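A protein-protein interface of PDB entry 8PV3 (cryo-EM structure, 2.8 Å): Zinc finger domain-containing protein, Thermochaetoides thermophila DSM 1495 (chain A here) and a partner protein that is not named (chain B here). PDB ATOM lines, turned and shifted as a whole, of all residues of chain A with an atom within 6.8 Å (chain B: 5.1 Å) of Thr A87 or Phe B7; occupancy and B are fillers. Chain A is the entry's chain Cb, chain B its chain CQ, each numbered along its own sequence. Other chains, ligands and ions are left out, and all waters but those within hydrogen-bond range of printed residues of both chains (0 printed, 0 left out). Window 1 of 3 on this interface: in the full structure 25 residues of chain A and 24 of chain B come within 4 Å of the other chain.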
ATOM      1  N   ASP A  18      28.192 -30.379  31.510  1.00  0.00           N
ATOM      2  CA  ASP A  18      28.427 -28.949  31.394  1.00  0.00           C
ATOM      3  C   ASP A  18      27.610 -28.190  32.439  1.00  0.00           C
ATOM      4  O   ASP A  18      26.590 -28.673  32.943  1.00  0.00           O
ATOM      5  CB  ASP A  18      28.081 -28.473  29.978  1.00  0.00           C
ATOM      6  CG  ASP A  18      28.599 -27.071  29.667  1.00  0.00           C
ATOM      7  OD1 ASP A  18      29.086 -26.368  30.579  1.00  0.00           O
ATOM      8  OD2 ASP A  18      28.516 -26.667  28.488  1.00  0.00           O
ATOM      9  N   ASP A  20      25.861 -25.358  32.269  1.00  0.00           N
ATOM     10  CA  ASP A  20      24.510 -24.947  31.892  1.00  0.00           C
ATOM     11  C   ASP A  20      23.548 -26.130  31.929  1.00  0.00           C
ATOM     12  O   ASP A  20      22.363 -25.968  32.253  1.00  0.00           O
ATOM     13  CB  ASP A  20      24.519 -24.282  30.513  1.00  0.00           C
ATOM     14  CG  ASP A  20      24.824 -25.253  29.392  1.00  0.00           C
ATOM     15  OD1 ASP A  20      25.659 -26.154  29.596  1.00  0.00           O
ATOM     16  OD2 ASP A  20      24.226 -25.114  28.304  1.00  0.00           O
ATOM     17  N   GLU A  23      22.666 -26.282  35.465  1.00  0.00           N
ATOM     18  CA  GLU A  23      21.646 -25.269  35.736  1.00  0.00           C
ATOM     19  C   GLU A  23      20.260 -25.762  35.345  1.00  0.00           C
ATOM     20  O   GLU A  23      19.291 -25.595  36.097  1.00  0.00           O
ATOM     21  CB  GLU A  23      21.966 -23.980  34.979  1.00  0.00           C
ATOM     22  CG  GLU A  23      22.960 -23.071  35.657  1.00  0.00           C
ATOM     23  CD  GLU A  23      22.882 -21.648  35.150  1.00  0.00           C
ATOM     24  OE1 GLU A  23      22.198 -21.415  34.130  1.00  0.00           O
ATOM     25  OE2 GLU A  23      23.505 -20.761  35.769  1.00  0.00           O
ATOM     26  N   ALA A  85      25.845 -19.865  34.774  1.00  0.00           N
ATOM     27  CA  ALA A  85      26.525 -20.488  33.651  1.00  0.00           C
ATOM     28  C   ALA A  85      26.375 -19.648  32.389  1.00  0.00           C
ATOM     29  O   ALA A  85      25.511 -18.773  32.292  1.00  0.00           O
ATOM     30  CB  ALA A  85      25.978 -21.892  33.412  1.00  0.00           C
ATOM     31  N   TYR A  86      27.236 -19.927  31.414  1.00  0.00           N
ATOM     32  CA  TYR A  86      27.239 -19.197  30.156  1.00  0.00           C
ATOM     33  C   TYR A  86      26.337 -19.888  29.141  1.00  0.00           C
ATOM     34  O   TYR A  86      26.435 -21.099  28.925  1.00  0.00           O
ATOM     35  CB  TYR A  86      28.664 -19.097  29.616  1.00  0.00           C
ATOM     36  CG  TYR A  86      28.824 -18.172  28.439  1.00  0.00           C
ATOM     37  CD1 TYR A  86      28.756 -16.797  28.598  1.00  0.00           C
ATOM     38  CD2 TYR A  86      29.051 -18.675  27.166  1.00  0.00           C
ATOM     39  CE1 TYR A  86      28.906 -15.951  27.522  1.00  0.00           C
ATOM     40  CE2 TYR A  86      29.203 -17.836  26.086  1.00  0.00           C
ATOM     41  CZ  TYR A  86      29.130 -16.476  26.268  1.00  0.00           C
ATOM     42  OH  TYR A  86      29.283 -15.638  25.191  1.00  0.00           O
ATOM     43  N   THR A  87      25.454 -19.112  28.515  1.00  0.00           N
ATOM     44  CA  THR A  87      24.442 -19.649  27.615  1.00  0.00           C
ATOM     45  C   THR A  87      24.444 -18.882  26.297  1.00  0.00           C
ATOM     46  O   THR A  87      25.159 -17.888  26.120  1.00  0.00           O
ATOM     47  CB  THR A  87      23.046 -19.600  28.252  1.00  0.00           C
ATOM     48  OG1 THR A  87      22.783 -18.276  28.730  1.00  0.00           O
ATOM     49  CG2 THR A  87      22.934 -20.588  29.402  1.00  0.00           C
ATOM     50  N   HIS A  88      23.611 -19.357  25.366  1.00  0.00           N
ATOM     51  CA  HIS A  88      23.479 -18.706  24.068  1.00  0.00           C
ATOM     52  C   HIS A  88      22.796 -17.350  24.183  1.00  0.00           C
ATOM     53  O   HIS A  88      23.066 -16.455  23.376  1.00  0.00           O
ATOM     54  CB  HIS A  88      22.708 -19.608  23.106  1.00  0.00           C
ATOM     55  CG  HIS A  88      23.563 -20.622  22.413  1.00  0.00           C
ATOM     56  ND1 HIS A  88      23.777 -21.885  22.918  1.00  0.00           N
ATOM     57  CD2 HIS A  88      24.256 -20.560  21.252  1.00  0.00           C
ATOM     58  CE1 HIS A  88      24.565 -22.558  22.099  1.00  0.00           C
ATOM     59  NE2 HIS A  88      24.869 -21.776  21.079  1.00  0.00           N
ATOM     60  N   GLU A  89      21.909 -17.180  25.168  1.00  0.00           N
ATOM     61  CA  GLU A  89      21.307 -15.870  25.405  1.00  0.00           C
ATOM     62  C   GLU A  89      22.355 -14.855  25.842  1.00  0.00           C
ATOM     63  O   GLU A  89      22.354 -13.711  25.373  1.00  0.00           O
ATOM     64  CB  GLU A  89      20.197 -15.980  26.449  1.00  0.00           C
ATOM     65  CG  GLU A  89      18.970 -16.746  25.980  1.00  0.00           C
ATOM     66  CD  GLU A  89      19.077 -18.236  26.232  1.00  0.00           C
ATOM     67  OE1 GLU A  89      20.073 -18.667  26.849  1.00  0.00           O
ATOM     68  OE2 GLU A  89      18.163 -18.977  25.814  1.00  0.00           O
ATOM     69  N   GLU A  90      23.270 -15.265  26.723  1.00  0.00           N
ATOM     70  CA  GLU A  90      24.373 -14.390  27.108  1.00  0.00           C
ATOM     71  C   GLU A  90      25.315 -14.151  25.934  1.00  0.00           C
ATOM     72  O   GLU A  90      25.870 -13.055  25.790  1.00  0.00           O
ATOM     73  CB  GLU A  90      25.125 -14.989  28.295  1.00  0.00           C
ATOM     74  CG  GLU A  90      26.163 -14.065  28.901  1.00  0.00           C
ATOM     75  CD  GLU A  90      26.486 -14.416  30.338  1.00  0.00           C
ATOM     76  OE1 GLU A  90      26.941 -13.523  31.082  1.00  0.00           O
ATOM     77  OE2 GLU A  90      26.285 -15.587  30.724  1.00  0.00           O
ATOM     78  N   ALA A  91      25.494 -15.162  25.078  1.00  0.00           N
ATOM     79  CA  ALA A  91      26.323 -14.994  23.888  1.00  0.00           C
ATOM     80  C   ALA A  91      25.733 -13.959  22.935  1.00  0.00           C
ATOM     81  O   ALA A  91      26.467 -13.150  22.354  1.00  0.00           O
ATOM     82  CB  ALA A  91      26.500 -16.336  23.181  1.00  0.00           C
ATOM     83  N   MET A  92      24.411 -13.974  22.752  1.00  0.00           N
ATOM     84  CA  MET A  92      23.771 -12.966  21.913  1.00  0.00           C
ATOM     85  C   MET A  92      23.813 -11.590  22.568  1.00  0.00           C
ATOM     86  O   MET A  92      24.013 -10.577  21.886  1.00  0.00           O
ATOM     87  CB  MET A  92      22.328 -13.361  21.602  1.00  0.00           C
ATOM     88  CG  MET A  92      22.184 -14.596  20.736  1.00  0.00           C
ATOM     89  SD  MET A  92      20.460 -14.961  20.355  1.00  0.00           S
ATOM     90  CE  MET A  92      19.892 -15.605  21.924  1.00  0.00           C
ATOM     91  N   ASN B   5      28.445 -15.946  14.651  1.00  0.00           N
ATOM     92  CA  ASN B   5      29.358 -15.422  15.652  1.00  0.00           C
ATOM     93  C   ASN B   5      29.819 -16.562  16.541  1.00  0.00           C
ATOM     94  O   ASN B   5      29.089 -17.534  16.757  1.00  0.00           O
ATOM     95  CB  ASN B   5      28.716 -14.320  16.489  1.00  0.00           C
ATOM     96  CG  ASN B   5      28.441 -13.070  15.686  1.00  0.00           C
ATOM     97  OD1 ASN B   5      29.273 -12.166  15.619  1.00  0.00           O
ATOM     98  ND2 ASN B   5      27.266 -13.008  15.075  1.00  0.00           N
ATOM     99  N   CYS B   6      31.050 -16.445  17.029  1.00  0.00           N
ATOM    100  CA  CYS B   6      31.607 -17.460  17.907  1.00  0.00           C
ATOM    101  C   CYS B   6      30.837 -17.494  19.219  1.00  0.00           C
ATOM    102  O   CYS B   6      30.490 -16.454  19.783  1.00  0.00           O
ATOM    103  CB  CYS B   6      33.085 -17.183  18.166  1.00  0.00           C
ATOM    104  SG  CYS B   6      33.890 -18.342  19.285  1.00  0.00           S
ATOM    105  N   PHE B   7      30.538 -18.706  19.683  1.00  0.00           N
ATOM    106  CA  PHE B   7      29.845 -18.868  20.954  1.00  0.00           C
ATOM    107  C   PHE B   7      30.703 -18.377  22.112  1.00  0.00           C
ATOM    108  O   PHE B   7      30.194 -17.757  23.051  1.00  0.00           O
ATOM    109  CB  PHE B   7      29.460 -20.336  21.142  1.00  0.00           C
ATOM    110  CG  PHE B   7      29.005 -20.678  22.528  1.00  0.00           C
ATOM    111  CD1 PHE B   7      27.734 -20.339  22.957  1.00  0.00           C
ATOM    112  CD2 PHE B   7      29.838 -21.365  23.395  1.00  0.00           C
ATOM    113  CE1 PHE B   7      27.311 -20.661  24.227  1.00  0.00           C
ATOM    114  CE2 PHE B   7      29.419 -21.687  24.668  1.00  0.00           C
ATOM    115  CZ  PHE B   7      28.153 -21.338  25.081  1.00  0.00           C
ATOM    116  N   PHE B   8      32.009 -18.630  22.051  1.00  0.00           N
ATOM    117  CA  PHE B   8      32.880 -18.358  23.186  1.00  0.00           C
ATOM    118  C   PHE B   8      33.278 -16.889  23.261  1.00  0.00           C
ATOM    119  O   PHE B   8      33.180 -16.270  24.325  1.00  0.00           O
ATOM    120  CB  PHE B   8      34.117 -19.252  23.109  1.00  0.00           C
ATOM    121  CG  PHE B   8      34.850 -19.382  24.407  1.00  0.00           C
ATOM    122  CD1 PHE B   8      35.889 -18.522  24.716  1.00  0.00           C
ATOM    123  CD2 PHE B   8      34.500 -20.358  25.322  1.00  0.00           C
ATOM    124  CE1 PHE B   8      36.563 -18.637  25.909  1.00  0.00           C
ATOM    125  CE2 PHE B   8      35.176 -20.476  26.518  1.00  0.00           C
ATOM    126  CZ  PHE B   8      36.204 -19.611  26.812  1.00  0.00           C
ATOM    127  N   CYS B   9      33.731 -16.312  22.149  1.00  0.00           N
ATOM    128  CA  CYS B   9      34.290 -14.969  22.161  1.00  0.00           C
ATOM    129  C   CYS B   9      33.478 -13.948  21.375  1.00  0.00           C
ATOM    130  O   CYS B   9      33.643 -12.747  21.608  1.00  0.00           O
ATOM    131  CB  CYS B   9      35.725 -14.987  21.620  1.00  0.00           C
ATOM    132  SG  CYS B   9      35.833 -15.098  19.832  1.00  0.00           S
ATOM    133  N   GLY B  10      32.617 -14.380  20.458  1.00  0.00           N
ATOM    134  CA  GLY B  10      31.764 -13.470  19.728  1.00  0.00           C
ATOM    135  C   GLY B  10      32.353 -12.884  18.464  1.00  0.00           C
ATOM    136  O   GLY B  10      31.726 -12.000  17.869  1.00  0.00           O
ATOM    137  N   PHE B  29      27.320 -25.567  19.177  1.00  0.00           N
ATOM    138  CA  PHE B  29      28.243 -24.551  19.673  1.00  0.00           C
ATOM    139  C   PHE B  29      29.267 -24.249  18.590  1.00  0.00           C
ATOM    140  O   PHE B  29      30.132 -25.079  18.310  1.00  0.00           O
ATOM    141  CB  PHE B  29      28.943 -25.017  20.951  1.00  0.00           C
ATOM    142  CG  PHE B  29      28.009 -25.316  22.087  1.00  0.00           C
ATOM    143  CD1 PHE B  29      27.434 -26.567  22.228  1.00  0.00           C
ATOM    144  CD2 PHE B  29      27.712 -24.341  23.017  1.00  0.00           C
ATOM    145  CE1 PHE B  29      26.578 -26.832  23.277  1.00  0.00           C
ATOM    146  CE2 PHE B  29      26.859 -24.599  24.062  1.00  0.00           C
ATOM    147  CZ  PHE B  29      26.291 -25.846  24.194  1.00  0.00           C
ATOM    148  N   ARG B  30      29.197 -23.059  18.003  1.00  0.00           N
ATOM    149  CA  ARG B  30      30.103 -22.683  16.927  1.00  0.00           C
ATOM    150  C   ARG B  30      31.282 -21.897  17.489  1.00  0.00           C
ATOM    151  O   ARG B  30      31.091 -20.928  18.230  1.00  0.00           O
ATOM    152  CB  ARG B  30      29.368 -21.859  15.870  1.00  0.00           C
ATOM    153  CG  ARG B  30      30.272 -21.255  14.812  1.00  0.00           C
ATOM    154  CD  ARG B  30      30.804 -22.322  13.880  1.00  0.00           C
ATOM    155  NE  ARG B  30      31.774 -21.802  12.927  1.00  0.00           N
ATOM    156  CZ  ARG B  30      31.468 -21.195  11.788  1.00  0.00           C
ATOM    157  NH1 ARG B  30      30.213 -21.033  11.406  1.00  0.00           N
ATOM    158  NH2 ARG B  30      32.447 -20.741  11.014  1.00  0.00           N
ATOM    159  N   PHE B  31      32.495 -22.315  17.142  1.00  0.00           N
ATOM    160  CA  PHE B  31      33.712 -21.637  17.545  1.00  0.00           C
ATOM    161  C   PHE B  31      34.474 -21.186  16.310  1.00  0.00           C
ATOM    162  O   PHE B  31      34.619 -21.936  15.342  1.00  0.00           O
ATOM    163  CB  PHE B  31      34.602 -22.546  18.394  1.00  0.00           C
ATOM    164  CG  PHE B  31      33.876 -23.215  19.509  1.00  0.00           C
ATOM    165  CD1 PHE B  31      33.499 -22.501  20.632  1.00  0.00           C
ATOM    166  CD2 PHE B  31      33.548 -24.554  19.427  1.00  0.00           C
ATOM    167  CE1 PHE B  31      32.816 -23.117  21.652  1.00  0.00           C
ATOM    168  CE2 PHE B  31      32.868 -25.170  20.442  1.00  0.00           C
ATOM    169  CZ  PHE B  31      32.498 -24.451  21.552  1.00  0.00           C
ATOM    170  N   PHE B  40      36.817 -23.784  25.577  1.00  0.00           N
ATOM    171  CA  PHE B  40      35.517 -24.378  25.873  1.00  0.00           C
ATOM    172  C   PHE B  40      35.658 -25.811  26.378  1.00  0.00           C
ATOM    173  O   PHE B  40      34.947 -26.219  27.303  1.00  0.00           O
ATOM    174  CB  PHE B  40      34.630 -24.331  24.631  1.00  0.00           C
ATOM    175  CG  PHE B  40      33.269 -24.935  24.830  1.00  0.00           C
ATOM    176  CD1 PHE B  40      32.257 -24.199  25.417  1.00  0.00           C
ATOM    177  CD2 PHE B  40      32.997 -26.232  24.423  1.00  0.00           C
ATOM    178  CE1 PHE B  40      31.008 -24.742  25.601  1.00  0.00           C
ATOM    179  CE2 PHE B  40      31.749 -26.778  24.606  1.00  0.00           C
ATOM    180  CZ  PHE B  40      30.754 -26.033  25.195  1.00  0.00           C
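Of the 11 printed residues of chain A, 4 touch a printed residue of chain B.
Printed residues of chain A that touch a printed residue of chain B: Tyr A86, Thr A87, His A88 and Ala A91.
Hydrophobic or aromatic side chains of chain A within 4 Å of the printed part of chain B: Tyr A86, His A88 and Ala A91.
Hydrophobic or aromatic side chains of chain B that line the printed part of chain A: Phe B7 and Phe B29.
Among the printed residues, 5 pairs touch across the chains.
Among the printed residues, no Asp or Glu carboxylate lies within 4 Å of a Lys or Arg side-chain nitrogen of the other chain.
Among the printed residues, pairs that only touch across the chains: Thr A87 with Phe B7 (3.96 Å), His A88 with Phe B7 (3.7 Å), His A88 with Phe B29 (3.6 Å) and Ala A91 with Phe B7 (3.96 Å).
The side-chain hydroxyl (OG1) of Thr A87 is in hydrogen-bond range of the side-chain carboxylate (OE1) of Glu A89 (3.3 Å).
The backbone NH (N) of Phe B7 sits at hydrogen-bond distance from the backbone carbonyl oxygen (O) of Arg B30 (2.7 Å).
The backbone carbonyl oxygen (O) of Phe B7 is in hydrogen-bond range of the side-chain hydroxyl (OH) of Tyr A86, at 3.1 Å.
Of chain B, only Phe B7 comes within 4 Å of Thr A87.
Printed residues of chain B within 4 Å of His A88: Phe B7 and Phe B29.
Of the printed residues of chain B, Tyr A86 touches Phe B7.
Of the printed residues of chain B, Ala A91 touches Phe B7 (3.96 Å).
Of the printed residues of chain A, Phe B29 touches His A88.
The nearest printed residue of chain A that does not touch Phe B7 is Asp A20 (6.3 Å).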
